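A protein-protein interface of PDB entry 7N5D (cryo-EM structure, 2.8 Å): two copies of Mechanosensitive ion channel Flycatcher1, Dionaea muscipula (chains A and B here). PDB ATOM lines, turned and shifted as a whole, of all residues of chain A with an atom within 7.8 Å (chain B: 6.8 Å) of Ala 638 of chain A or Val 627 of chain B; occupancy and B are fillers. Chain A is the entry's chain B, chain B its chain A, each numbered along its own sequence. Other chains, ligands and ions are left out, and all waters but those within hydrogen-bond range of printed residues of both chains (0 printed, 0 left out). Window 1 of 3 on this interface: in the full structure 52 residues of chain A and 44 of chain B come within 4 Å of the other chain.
N of Asn 641 of chain A is in hydrogen-bond range of O of Lys 626 of chain B (2.9 Å). The side-chain hydroxyl of Ser 645 of chain A lies within hydrogen-bond range of the backbone NH of Lys 626 of chain B, at 2.9 Å. The backbone NH (N) of Tyr 628 of chain B sits at hydrogen-bond distance from the backbone carbonyl oxygen (O) of Ile 639 of chain A, 3.0 Å away.
The backbone NH (N) of Val 627 of chain B lies within hydrogen-bond range of the backbone carbonyl oxygen (O) of Phe 619 of chain B, at 2.8 Å. The side-chain amino group of Lys 621 of chain B is in salt-bridge range of the side-chain carboxylate of Glu 625 of chain B (3.97 Å). The backbone carbonyl oxygen of Gly 640 of chain A lies within hydrogen-bond range of the backbone NH of Val 601 of chain A, at 2.8 Å. The side-chain amino group (NZ) of Lys 637 of chain A lies within salt-bridge range of the side-chain carboxylate (OD2) of Asp 603 of chain A, at 2.9 Å. The backbone carbonyl oxygen (O) of Ile 633 of chain A lies within hydrogen-bond range of the side-chain hydroxyl (OG1) of Thr 636 of chain A, 3.0 Å away. The side-chain hydroxyl of Ser 645 of chain A is in hydrogen-bond range of the backbone carbonyl oxygen of Asn 641 of chain A, at 2.7 Å.
Among the printed residues, pairs that only touch across the chains: Thr 636 of chain A with Ile 633 of chain B (3.0 Å), Phe 642 of chain A with Glu 625 of chain B (3.2 Å), Gly 640 of chain A with Lys 626 of chain B (3.3 Å), Ala 638 of chain A with Tyr 628 of chain B (3.3 Å), Lys 637 of chain A with Pro 630 of chain B (3.6 Å), Ile 639 of chain A with Val 627 of chain B (3.6 Å), Val 601 of chain A with Glu 625 of chain B (3.6 Å), Ala 638 of chain A with Tyr 629 of chain B (3.6 Å), Ser 645 of chain A with Glu 625 of chain B (3.6 Å), Gly 640 of chain A with Glu 625 of chain B (3.7 Å), Ser 645 of chain A with Lys 624 of chain B (3.7 Å), Ile 639 of chain A with Lys 626 of chain B (3.8 Å), Pro 593 of chain A with Tyr 628 of chain B (3.8 Å), Cys 635 of chain A with Pro 630 of chain B (3.9 Å), Lys 637 of chain A with Tyr 628 of chain B (3.9 Å) and Ala 638 of chain A with Val 627 of chain B (3.98 Å).
Of the printed residues of chain B, Pro 593 of chain A touches Tyr 628. Asp 603 of chain A touches none of the printed residues of chain B. Printed residues of chain B within 4 Å of Ala 638 of chain A: Val 627 (3.98 Å), Tyr 628 (3.3 Å) and Tyr 629 (3.6 Å). Of the printed residues of chain A, Val 627 of chain B touches Ala 638 (3.98 Å) and Ile 639 (3.6 Å). Of the printed residues of chain A, Ile 633 of chain B touches Thr 636 (3.0 Å). The nearest printed residue of chain A that does not touch Val 627 of chain B is Gly 640 of chain A (4.3 Å).
Of the 16 printed residues of chain A, 11 touch a printed residue of chain B. Of the 15 printed residues of chain B, 8 touch a printed residue of chain A. Hydrophobic or aromatic side chains of chain B that line the printed part of chain A: Val 627, Tyr 628, Tyr 629, Pro 630 and Ile 633.
1 position is printed for both chains.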
ATOM      1  N   PRO A 593      -8.637   2.288   5.499  1.00  0.00           N
ATOM      2  CA  PRO A 593      -8.467   1.407   4.353  1.00  0.00           C
ATOM      3  C   PRO A 593      -9.524   0.322   4.185  1.00  0.00           C
ATOM      4  O   PRO A 593      -9.615  -0.279   3.117  1.00  0.00           O
ATOM      5  CB  PRO A 593      -7.108   0.792   4.619  1.00  0.00           C
ATOM      6  CG  PRO A 593      -6.932   0.883   6.093  1.00  0.00           C
ATOM      7  CD  PRO A 593      -7.591   2.142   6.502  1.00  0.00           C
ATOM      8  N   VAL A 601      -6.496  -7.620   1.149  1.00  0.00           N
ATOM      9  CA  VAL A 601      -5.317  -8.425   0.917  1.00  0.00           C
ATOM     10  C   VAL A 601      -4.112  -7.828   1.621  1.00  0.00           C
ATOM     11  O   VAL A 601      -3.698  -6.703   1.332  1.00  0.00           O
ATOM     12  CB  VAL A 601      -5.034  -8.525  -0.571  1.00  0.00           C
ATOM     13  CG1 VAL A 601      -3.847  -9.427  -0.792  1.00  0.00           C
ATOM     14  CG2 VAL A 601      -6.260  -8.975  -1.270  1.00  0.00           C
ATOM     15  N   ILE A 602      -3.553  -8.570   2.562  1.00  0.00           N
ATOM     16  CA  ILE A 602      -2.413  -8.082   3.324  1.00  0.00           C
ATOM     17  C   ILE A 602      -1.255  -9.042   3.187  1.00  0.00           C
ATOM     18  O   ILE A 602      -1.357 -10.197   3.567  1.00  0.00           O
ATOM     19  CB  ILE A 602      -2.821  -7.887   4.784  1.00  0.00           C
ATOM     20  CG1 ILE A 602      -3.981  -6.877   4.823  1.00  0.00           C
ATOM     21  CG2 ILE A 602      -1.645  -7.428   5.622  1.00  0.00           C
ATOM     22  CD1 ILE A 602      -4.640  -6.710   6.119  1.00  0.00           C
ATOM     23  N   ASP A 603      -0.145  -8.588   2.634  1.00  0.00           N
ATOM     24  CA  ASP A 603       1.024  -9.435   2.407  1.00  0.00           C
ATOM     25  C   ASP A 603       0.679 -10.706   1.640  1.00  0.00           C
ATOM     26  O   ASP A 603       1.193 -11.784   1.921  1.00  0.00           O
ATOM     27  CB  ASP A 603       1.702  -9.791   3.723  1.00  0.00           C
ATOM     28  CG  ASP A 603       2.285  -8.576   4.438  1.00  0.00           C
ATOM     29  OD1 ASP A 603       2.708  -7.648   3.780  1.00  0.00           O
ATOM     30  OD2 ASP A 603       2.308  -8.579   5.656  1.00  0.00           O
ATOM     31  N   GLY A 604      -0.212 -10.575   0.676  1.00  0.00           N
ATOM     32  CA  GLY A 604      -0.634 -11.683  -0.167  1.00  0.00           C
ATOM     33  C   GLY A 604      -1.751 -12.547   0.427  1.00  0.00           C
ATOM     34  O   GLY A 604      -2.254 -13.446  -0.250  1.00  0.00           O
ATOM     35  N   ILE A 633       1.065  -2.477  13.158  1.00  0.00           N
ATOM     36  CA  ILE A 633       1.811  -3.053  12.059  1.00  0.00           C
ATOM     37  C   ILE A 633       1.005  -2.832  10.780  1.00  0.00           C
ATOM     38  O   ILE A 633       1.568  -2.602   9.722  1.00  0.00           O
ATOM     39  CB  ILE A 633       2.237  -4.518  12.284  1.00  0.00           C
ATOM     40  CG1 ILE A 633       1.044  -5.499  12.352  1.00  0.00           C
ATOM     41  CG2 ILE A 633       3.035  -4.550  13.589  1.00  0.00           C
ATOM     42  CD1 ILE A 633       1.443  -6.990  12.327  1.00  0.00           C
ATOM     43  N   LEU A 634      -0.333  -2.839  10.859  1.00  0.00           N
ATOM     44  CA  LEU A 634      -1.123  -2.596   9.648  1.00  0.00           C
ATOM     45  C   LEU A 634      -0.897  -1.195   9.120  1.00  0.00           C
ATOM     46  O   LEU A 634      -0.936  -0.964   7.912  1.00  0.00           O
ATOM     47  CB  LEU A 634      -2.611  -2.764   9.881  1.00  0.00           C
ATOM     48  CG  LEU A 634      -3.117  -4.125  10.147  1.00  0.00           C
ATOM     49  CD1 LEU A 634      -4.543  -4.030  10.500  1.00  0.00           C
ATOM     50  CD2 LEU A 634      -2.979  -4.978   8.946  1.00  0.00           C
ATOM     51  N   CYS A 635      -0.575  -0.272  10.009  1.00  0.00           N
ATOM     52  CA  CYS A 635      -0.304   1.109   9.664  1.00  0.00           C
ATOM     53  C   CYS A 635       0.871   1.259   8.726  1.00  0.00           C
ATOM     54  O   CYS A 635       1.074   2.337   8.177  1.00  0.00           O
ATOM     55  CB  CYS A 635       0.069   1.923  10.893  1.00  0.00           C
ATOM     56  SG  CYS A 635      -1.200   2.156  12.073  1.00  0.00           S
ATOM     57  N   THR A 636       1.690   0.228   8.577  1.00  0.00           N
ATOM     58  CA  THR A 636       2.837   0.307   7.717  1.00  0.00           C
ATOM     59  C   THR A 636       2.738  -0.648   6.541  1.00  0.00           C
ATOM     60  O   THR A 636       3.759  -1.024   5.963  1.00  0.00           O
ATOM     61  CB  THR A 636       4.139   0.014   8.456  1.00  0.00           C
ATOM     62  OG1 THR A 636       4.118  -1.297   8.980  1.00  0.00           O
ATOM     63  CG2 THR A 636       4.265   0.974   9.593  1.00  0.00           C
ATOM     64  N   LYS A 637       1.547  -1.128   6.230  1.00  0.00           N
ATOM     65  CA  LYS A 637       1.396  -2.048   5.120  1.00  0.00           C
ATOM     66  C   LYS A 637       0.547  -1.504   4.005  1.00  0.00           C
ATOM     67  O   LYS A 637      -0.335  -0.679   4.225  1.00  0.00           O
ATOM     68  CB  LYS A 637       0.792  -3.342   5.614  1.00  0.00           C
ATOM     69  CG  LYS A 637       1.676  -4.055   6.546  1.00  0.00           C
ATOM     70  CD  LYS A 637       1.085  -5.341   7.009  1.00  0.00           C
ATOM     71  CE  LYS A 637       1.964  -5.996   8.032  1.00  0.00           C
ATOM     72  NZ  LYS A 637       3.210  -6.515   7.420  1.00  0.00           N
ATOM     73  N   ALA A 638       0.793  -1.985   2.797  1.00  0.00           N
ATOM     74  CA  ALA A 638      -0.070  -1.648   1.682  1.00  0.00           C
ATOM     75  C   ALA A 638      -1.229  -2.617   1.727  1.00  0.00           C
ATOM     76  O   ALA A 638      -1.024  -3.829   1.751  1.00  0.00           O
ATOM     77  CB  ALA A 638       0.672  -1.714   0.376  1.00  0.00           C
ATOM     78  N   ILE A 639      -2.437  -2.103   1.793  1.00  0.00           N
ATOM     79  CA  ILE A 639      -3.592  -2.964   1.963  1.00  0.00           C
ATOM     80  C   ILE A 639      -4.522  -2.982   0.772  1.00  0.00           C
ATOM     81  O   ILE A 639      -5.051  -1.945   0.370  1.00  0.00           O
ATOM     82  CB  ILE A 639      -4.352  -2.520   3.233  1.00  0.00           C
ATOM     83  CG1 ILE A 639      -3.387  -2.652   4.444  1.00  0.00           C
ATOM     84  CG2 ILE A 639      -5.631  -3.321   3.427  1.00  0.00           C
ATOM     85  CD1 ILE A 639      -3.872  -2.097   5.736  1.00  0.00           C
ATOM     86  N   GLY A 640      -4.746  -4.164   0.206  1.00  0.00           N
ATOM     87  CA  GLY A 640      -5.661  -4.271  -0.913  1.00  0.00           C
ATOM     88  C   GLY A 640      -7.061  -4.335  -0.355  1.00  0.00           C
ATOM     89  O   GLY A 640      -7.270  -4.959   0.675  1.00  0.00           O
ATOM     90  N   ASN A 641      -8.039  -3.839  -1.077  1.00  0.00           N
ATOM     91  CA  ASN A 641      -9.425  -3.931  -0.648  1.00  0.00           C
ATOM     92  C   ASN A 641     -10.299  -4.309  -1.827  1.00  0.00           C
ATOM     93  O   ASN A 641     -10.533  -3.494  -2.714  1.00  0.00           O
ATOM     94  CB  ASN A 641      -9.871  -2.641   0.006  1.00  0.00           C
ATOM     95  CG  ASN A 641     -11.226  -2.737   0.568  1.00  0.00           C
ATOM     96  OD1 ASN A 641     -12.133  -3.281  -0.075  1.00  0.00           O
ATOM     97  ND2 ASN A 641     -11.422  -2.216   1.753  1.00  0.00           N
ATOM     98  N   PHE A 642     -10.767  -5.554  -1.855  1.00  0.00           N
ATOM     99  CA  PHE A 642     -11.559  -6.043  -2.970  1.00  0.00           C
ATOM    100  C   PHE A 642     -12.934  -5.439  -2.967  1.00  0.00           C
ATOM    101  O   PHE A 642     -13.458  -5.073  -4.001  1.00  0.00           O
ATOM    102  CB  PHE A 642     -11.739  -7.538  -2.906  1.00  0.00           C
ATOM    103  CG  PHE A 642     -10.566  -8.383  -3.194  1.00  0.00           C
ATOM    104  CD1 PHE A 642     -10.491  -9.562  -2.581  1.00  0.00           C
ATOM    105  CD2 PHE A 642      -9.581  -8.053  -4.063  1.00  0.00           C
ATOM    106  CE1 PHE A 642      -9.479 -10.418  -2.803  1.00  0.00           C
ATOM    107  CE2 PHE A 642      -8.567  -8.904  -4.293  1.00  0.00           C
ATOM    108  CZ  PHE A 642      -8.517 -10.087  -3.664  1.00  0.00           C
ATOM    109  N   SER A 645     -13.016  -2.305  -4.828  1.00  0.00           N
ATOM    110  CA  SER A 645     -12.440  -2.374  -6.158  1.00  0.00           C
ATOM    111  C   SER A 645     -13.493  -2.386  -7.267  1.00  0.00           C
ATOM    112  O   SER A 645     -14.623  -2.834  -7.068  1.00  0.00           O
ATOM    113  CB  SER A 645     -11.570  -3.612  -6.263  1.00  0.00           C
ATOM    114  OG  SER A 645     -10.446  -3.508  -5.431  1.00  0.00           O
ATOM    115  N   MET B 607       1.336  -0.073 -11.333  1.00  0.00           N
ATOM    116  CA  MET B 607       0.071   0.366 -10.788  1.00  0.00           C
ATOM    117  C   MET B 607      -0.347   1.731 -11.273  1.00  0.00           C
ATOM    118  O   MET B 607       0.475   2.607 -11.497  1.00  0.00           O
ATOM    119  CB  MET B 607       0.141   0.396  -9.288  1.00  0.00           C
ATOM    120  CG  MET B 607       0.503  -0.908  -8.651  1.00  0.00           C
ATOM    121  SD  MET B 607       0.399  -0.880  -6.881  1.00  0.00           S
ATOM    122  CE  MET B 607       1.842   0.001  -6.468  1.00  0.00           C
ATOM    123  N   GLU B 610      -4.724   6.244  -8.610  1.00  0.00           N
ATOM    124  CA  GLU B 610      -6.109   6.623  -8.639  1.00  0.00           C
ATOM    125  C   GLU B 610      -6.345   7.912  -7.908  1.00  0.00           C
ATOM    126  O   GLU B 610      -7.021   8.796  -8.408  1.00  0.00           O
ATOM    127  CB  GLU B 610      -6.977   5.556  -8.018  1.00  0.00           C
ATOM    128  CG  GLU B 610      -8.427   5.863  -8.122  1.00  0.00           C
ATOM    129  CD  GLU B 610      -9.298   4.828  -7.537  1.00  0.00           C
ATOM    130  OE1 GLU B 610      -8.815   3.801  -7.149  1.00  0.00           O
ATOM    131  OE2 GLU B 610     -10.482   5.069  -7.425  1.00  0.00           O
ATOM    132  N   THR B 617      -1.726   7.187  -0.710  1.00  0.00           N
ATOM    133  CA  THR B 617      -1.916   7.213  -2.141  1.00  0.00           C
ATOM    134  C   THR B 617      -2.691   5.963  -2.490  1.00  0.00           C
ATOM    135  O   THR B 617      -2.445   4.895  -1.926  1.00  0.00           O
ATOM    136  CB  THR B 617      -0.599   7.272  -2.921  1.00  0.00           C
ATOM    137  OG1 THR B 617       0.113   8.466  -2.570  1.00  0.00           O
ATOM    138  CG2 THR B 617      -0.891   7.295  -4.425  1.00  0.00           C
ATOM    139  N   VAL B 618      -3.679   6.087  -3.350  1.00  0.00           N
ATOM    140  CA  VAL B 618      -4.460   4.930  -3.727  1.00  0.00           C
ATOM    141  C   VAL B 618      -4.117   4.522  -5.131  1.00  0.00           C
ATOM    142  O   VAL B 618      -4.183   5.339  -6.048  1.00  0.00           O
ATOM    143  CB  VAL B 618      -5.943   5.212  -3.604  1.00  0.00           C
ATOM    144  CG1 VAL B 618      -6.736   4.011  -4.008  1.00  0.00           C
ATOM    145  CG2 VAL B 618      -6.241   5.587  -2.209  1.00  0.00           C
ATOM    146  N   PHE B 619      -3.746   3.265  -5.288  1.00  0.00           N
ATOM    147  CA  PHE B 619      -3.325   2.706  -6.560  1.00  0.00           C
ATOM    148  C   PHE B 619      -4.170   1.549  -7.057  1.00  0.00           C
ATOM    149  O   PHE B 619      -4.728   0.796  -6.274  1.00  0.00           O
ATOM    150  CB  PHE B 619      -1.926   2.141  -6.446  1.00  0.00           C
ATOM    151  CG  PHE B 619      -0.839   3.054  -6.186  1.00  0.00           C
ATOM    152  CD1 PHE B 619      -0.443   3.316  -4.916  1.00  0.00           C
ATOM    153  CD2 PHE B 619      -0.169   3.627  -7.210  1.00  0.00           C
ATOM    154  CE1 PHE B 619       0.595   4.144  -4.678  1.00  0.00           C
ATOM    155  CE2 PHE B 619       0.872   4.456  -6.968  1.00  0.00           C
ATOM    156  CZ  PHE B 619       1.246   4.715  -5.703  1.00  0.00           C
ATOM    157  N   LEU B 620      -4.221   1.353  -8.361  1.00  0.00           N
ATOM    158  CA  LEU B 620      -4.862   0.168  -8.922  1.00  0.00           C
ATOM    159  C   LEU B 620      -3.849  -0.750  -9.554  1.00  0.00           C
ATOM    160  O   LEU B 620      -3.054  -0.353 -10.404  1.00  0.00           O
ATOM    161  CB  LEU B 620      -5.897   0.515  -9.993  1.00  0.00           C
ATOM    162  CG  LEU B 620      -7.150   1.279  -9.593  1.00  0.00           C
ATOM    163  CD1 LEU B 620      -7.893   1.656 -10.830  1.00  0.00           C
ATOM    164  CD2 LEU B 620      -8.047   0.407  -8.745  1.00  0.00           C
ATOM    165  N   LYS B 621      -3.904  -2.004  -9.188  1.00  0.00           N
ATOM    166  CA  LYS B 621      -2.974  -2.984  -9.724  1.00  0.00           C
ATOM    167  C   LYS B 621      -3.410  -3.412 -11.103  1.00  0.00           C
ATOM    168  O   LYS B 621      -4.462  -3.001 -11.578  1.00  0.00           O
ATOM    169  CB  LYS B 621      -2.859  -4.170  -8.799  1.00  0.00           C
ATOM    170  CG  LYS B 621      -2.253  -3.834  -7.468  1.00  0.00           C
ATOM    171  CD  LYS B 621      -2.241  -5.029  -6.532  1.00  0.00           C
ATOM    172  CE  LYS B 621      -1.141  -6.015  -6.826  1.00  0.00           C
ATOM    173  NZ  LYS B 621      -1.219  -7.180  -5.899  1.00  0.00           N
ATOM    174  N   LYS B 624      -6.821  -4.540 -11.268  1.00  0.00           N
ATOM    175  CA  LYS B 624      -7.651  -3.504 -10.714  1.00  0.00           C
ATOM    176  C   LYS B 624      -7.971  -3.659  -9.245  1.00  0.00           C
ATOM    177  O   LYS B 624      -8.924  -3.061  -8.756  1.00  0.00           O
ATOM    178  CB  LYS B 624      -8.958  -3.409 -11.468  1.00  0.00           C
ATOM    179  CG  LYS B 624      -8.857  -3.407 -12.970  1.00  0.00           C
ATOM    180  CD  LYS B 624      -8.200  -2.175 -13.516  1.00  0.00           C
ATOM    181  CE  LYS B 624      -8.025  -2.290 -15.017  1.00  0.00           C
ATOM    182  NZ  LYS B 624      -9.318  -2.488 -15.736  1.00  0.00           N
ATOM    183  N   GLU B 625      -7.141  -4.371  -8.507  1.00  0.00           N
ATOM    184  CA  GLU B 625      -7.305  -4.377  -7.070  1.00  0.00           C
ATOM    185  C   GLU B 625      -6.966  -2.991  -6.566  1.00  0.00           C
ATOM    186  O   GLU B 625      -5.955  -2.412  -6.970  1.00  0.00           O
ATOM    187  CB  GLU B 625      -6.361  -5.370  -6.419  1.00  0.00           C
ATOM    188  CG  GLU B 625      -6.455  -5.494  -4.899  1.00  0.00           C
ATOM    189  CD  GLU B 625      -5.444  -6.472  -4.385  1.00  0.00           C
ATOM    190  OE1 GLU B 625      -5.656  -7.642  -4.519  1.00  0.00           O
ATOM    191  OE2 GLU B 625      -4.438  -6.041  -3.871  1.00  0.00           O
ATOM    192  N   LYS B 626      -7.778  -2.453  -5.673  1.00  0.00           N
ATOM    193  CA  LYS B 626      -7.507  -1.150  -5.088  1.00  0.00           C
ATOM    194  C   LYS B 626      -6.591  -1.281  -3.901  1.00  0.00           C
ATOM    195  O   LYS B 626      -6.872  -2.026  -2.970  1.00  0.00           O
ATOM    196  CB  LYS B 626      -8.798  -0.484  -4.659  1.00  0.00           C
ATOM    197  CG  LYS B 626      -8.633   0.942  -4.212  1.00  0.00           C
ATOM    198  CD  LYS B 626      -9.891   1.486  -3.608  1.00  0.00           C
ATOM    199  CE  LYS B 626     -10.986   1.785  -4.594  1.00  0.00           C
ATOM    200  NZ  LYS B 626     -10.763   3.007  -5.321  1.00  0.00           N
ATOM    201  N   VAL B 627      -5.500  -0.533  -3.914  1.00  0.00           N
ATOM    202  CA  VAL B 627      -4.495  -0.583  -2.869  1.00  0.00           C
ATOM    203  C   VAL B 627      -4.249   0.718  -2.152  1.00  0.00           C
ATOM    204  O   VAL B 627      -3.927   1.732  -2.765  1.00  0.00           O
ATOM    205  CB  VAL B 627      -3.165  -1.024  -3.483  1.00  0.00           C
ATOM    206  CG1 VAL B 627      -2.066  -1.056  -2.438  1.00  0.00           C
ATOM    207  CG2 VAL B 627      -3.336  -2.347  -4.105  1.00  0.00           C
ATOM    208  N   TYR B 628      -4.339   0.670  -0.842  1.00  0.00           N
ATOM    209  CA  TYR B 628      -4.068   1.824  -0.013  1.00  0.00           C
ATOM    210  C   TYR B 628      -2.636   1.741   0.421  1.00  0.00           C
ATOM    211  O   TYR B 628      -2.239   0.819   1.131  1.00  0.00           O
ATOM    212  CB  TYR B 628      -5.008   1.837   1.161  1.00  0.00           C
ATOM    213  CG  TYR B 628      -6.362   2.100   0.733  1.00  0.00           C
ATOM    214  CD1 TYR B 628      -7.161   1.088   0.281  1.00  0.00           C
ATOM    215  CD2 TYR B 628      -6.820   3.351   0.783  1.00  0.00           C
ATOM    216  CE1 TYR B 628      -8.412   1.364  -0.126  1.00  0.00           C
ATOM    217  CE2 TYR B 628      -8.070   3.623   0.382  1.00  0.00           C
ATOM    218  CZ  TYR B 628      -8.857   2.644  -0.070  1.00  0.00           C
ATOM    219  OH  TYR B 628     -10.119   2.940  -0.464  1.00  0.00           O
ATOM    220  N   TYR B 629      -1.840   2.698  -0.011  1.00  0.00           N
ATOM    221  CA  TYR B 629      -0.415   2.646   0.205  1.00  0.00           C
ATOM    222  C   TYR B 629       0.059   3.891   0.971  1.00  0.00           C
ATOM    223  O   TYR B 629       0.029   4.983   0.405  1.00  0.00           O
ATOM    224  CB  TYR B 629       0.219   2.605  -1.155  1.00  0.00           C
ATOM    225  CG  TYR B 629       1.515   2.062  -1.199  1.00  0.00           C
ATOM    226  CD1 TYR B 629       1.652   0.924  -1.908  1.00  0.00           C
ATOM    227  CD2 TYR B 629       2.557   2.598  -0.556  1.00  0.00           C
ATOM    228  CE1 TYR B 629       2.820   0.326  -1.988  1.00  0.00           C
ATOM    229  CE2 TYR B 629       3.744   1.986  -0.631  1.00  0.00           C
ATOM    230  CZ  TYR B 629       3.866   0.852  -1.350  1.00  0.00           C
ATOM    231  OH  TYR B 629       5.052   0.237  -1.429  1.00  0.00           O
ATOM    232  N   PRO B 630       0.436   3.804   2.253  1.00  0.00           N
ATOM    233  CA  PRO B 630       0.813   4.920   3.090  1.00  0.00           C
ATOM    234  C   PRO B 630       1.936   5.733   2.508  1.00  0.00           C
ATOM    235  O   PRO B 630       2.934   5.181   2.035  1.00  0.00           O
ATOM    236  CB  PRO B 630       1.286   4.222   4.349  1.00  0.00           C
ATOM    237  CG  PRO B 630       0.557   2.937   4.353  1.00  0.00           C
ATOM    238  CD  PRO B 630       0.482   2.528   2.928  1.00  0.00           C
ATOM    239  N   ILE B 633       5.666   5.335   3.732  1.00  0.00           N
ATOM    240  CA  ILE B 633       6.438   4.246   3.187  1.00  0.00           C
ATOM    241  C   ILE B 633       6.850   4.581   1.794  1.00  0.00           C
ATOM    242  O   ILE B 633       7.962   4.315   1.363  1.00  0.00           O
ATOM    243  CB  ILE B 633       5.646   2.977   3.171  1.00  0.00           C
ATOM    244  CG1 ILE B 633       5.384   2.633   4.548  1.00  0.00           C
ATOM    245  CG2 ILE B 633       6.387   1.893   2.407  1.00  0.00           C
ATOM    246  CD1 ILE B 633       4.435   1.601   4.713  1.00  0.00           C
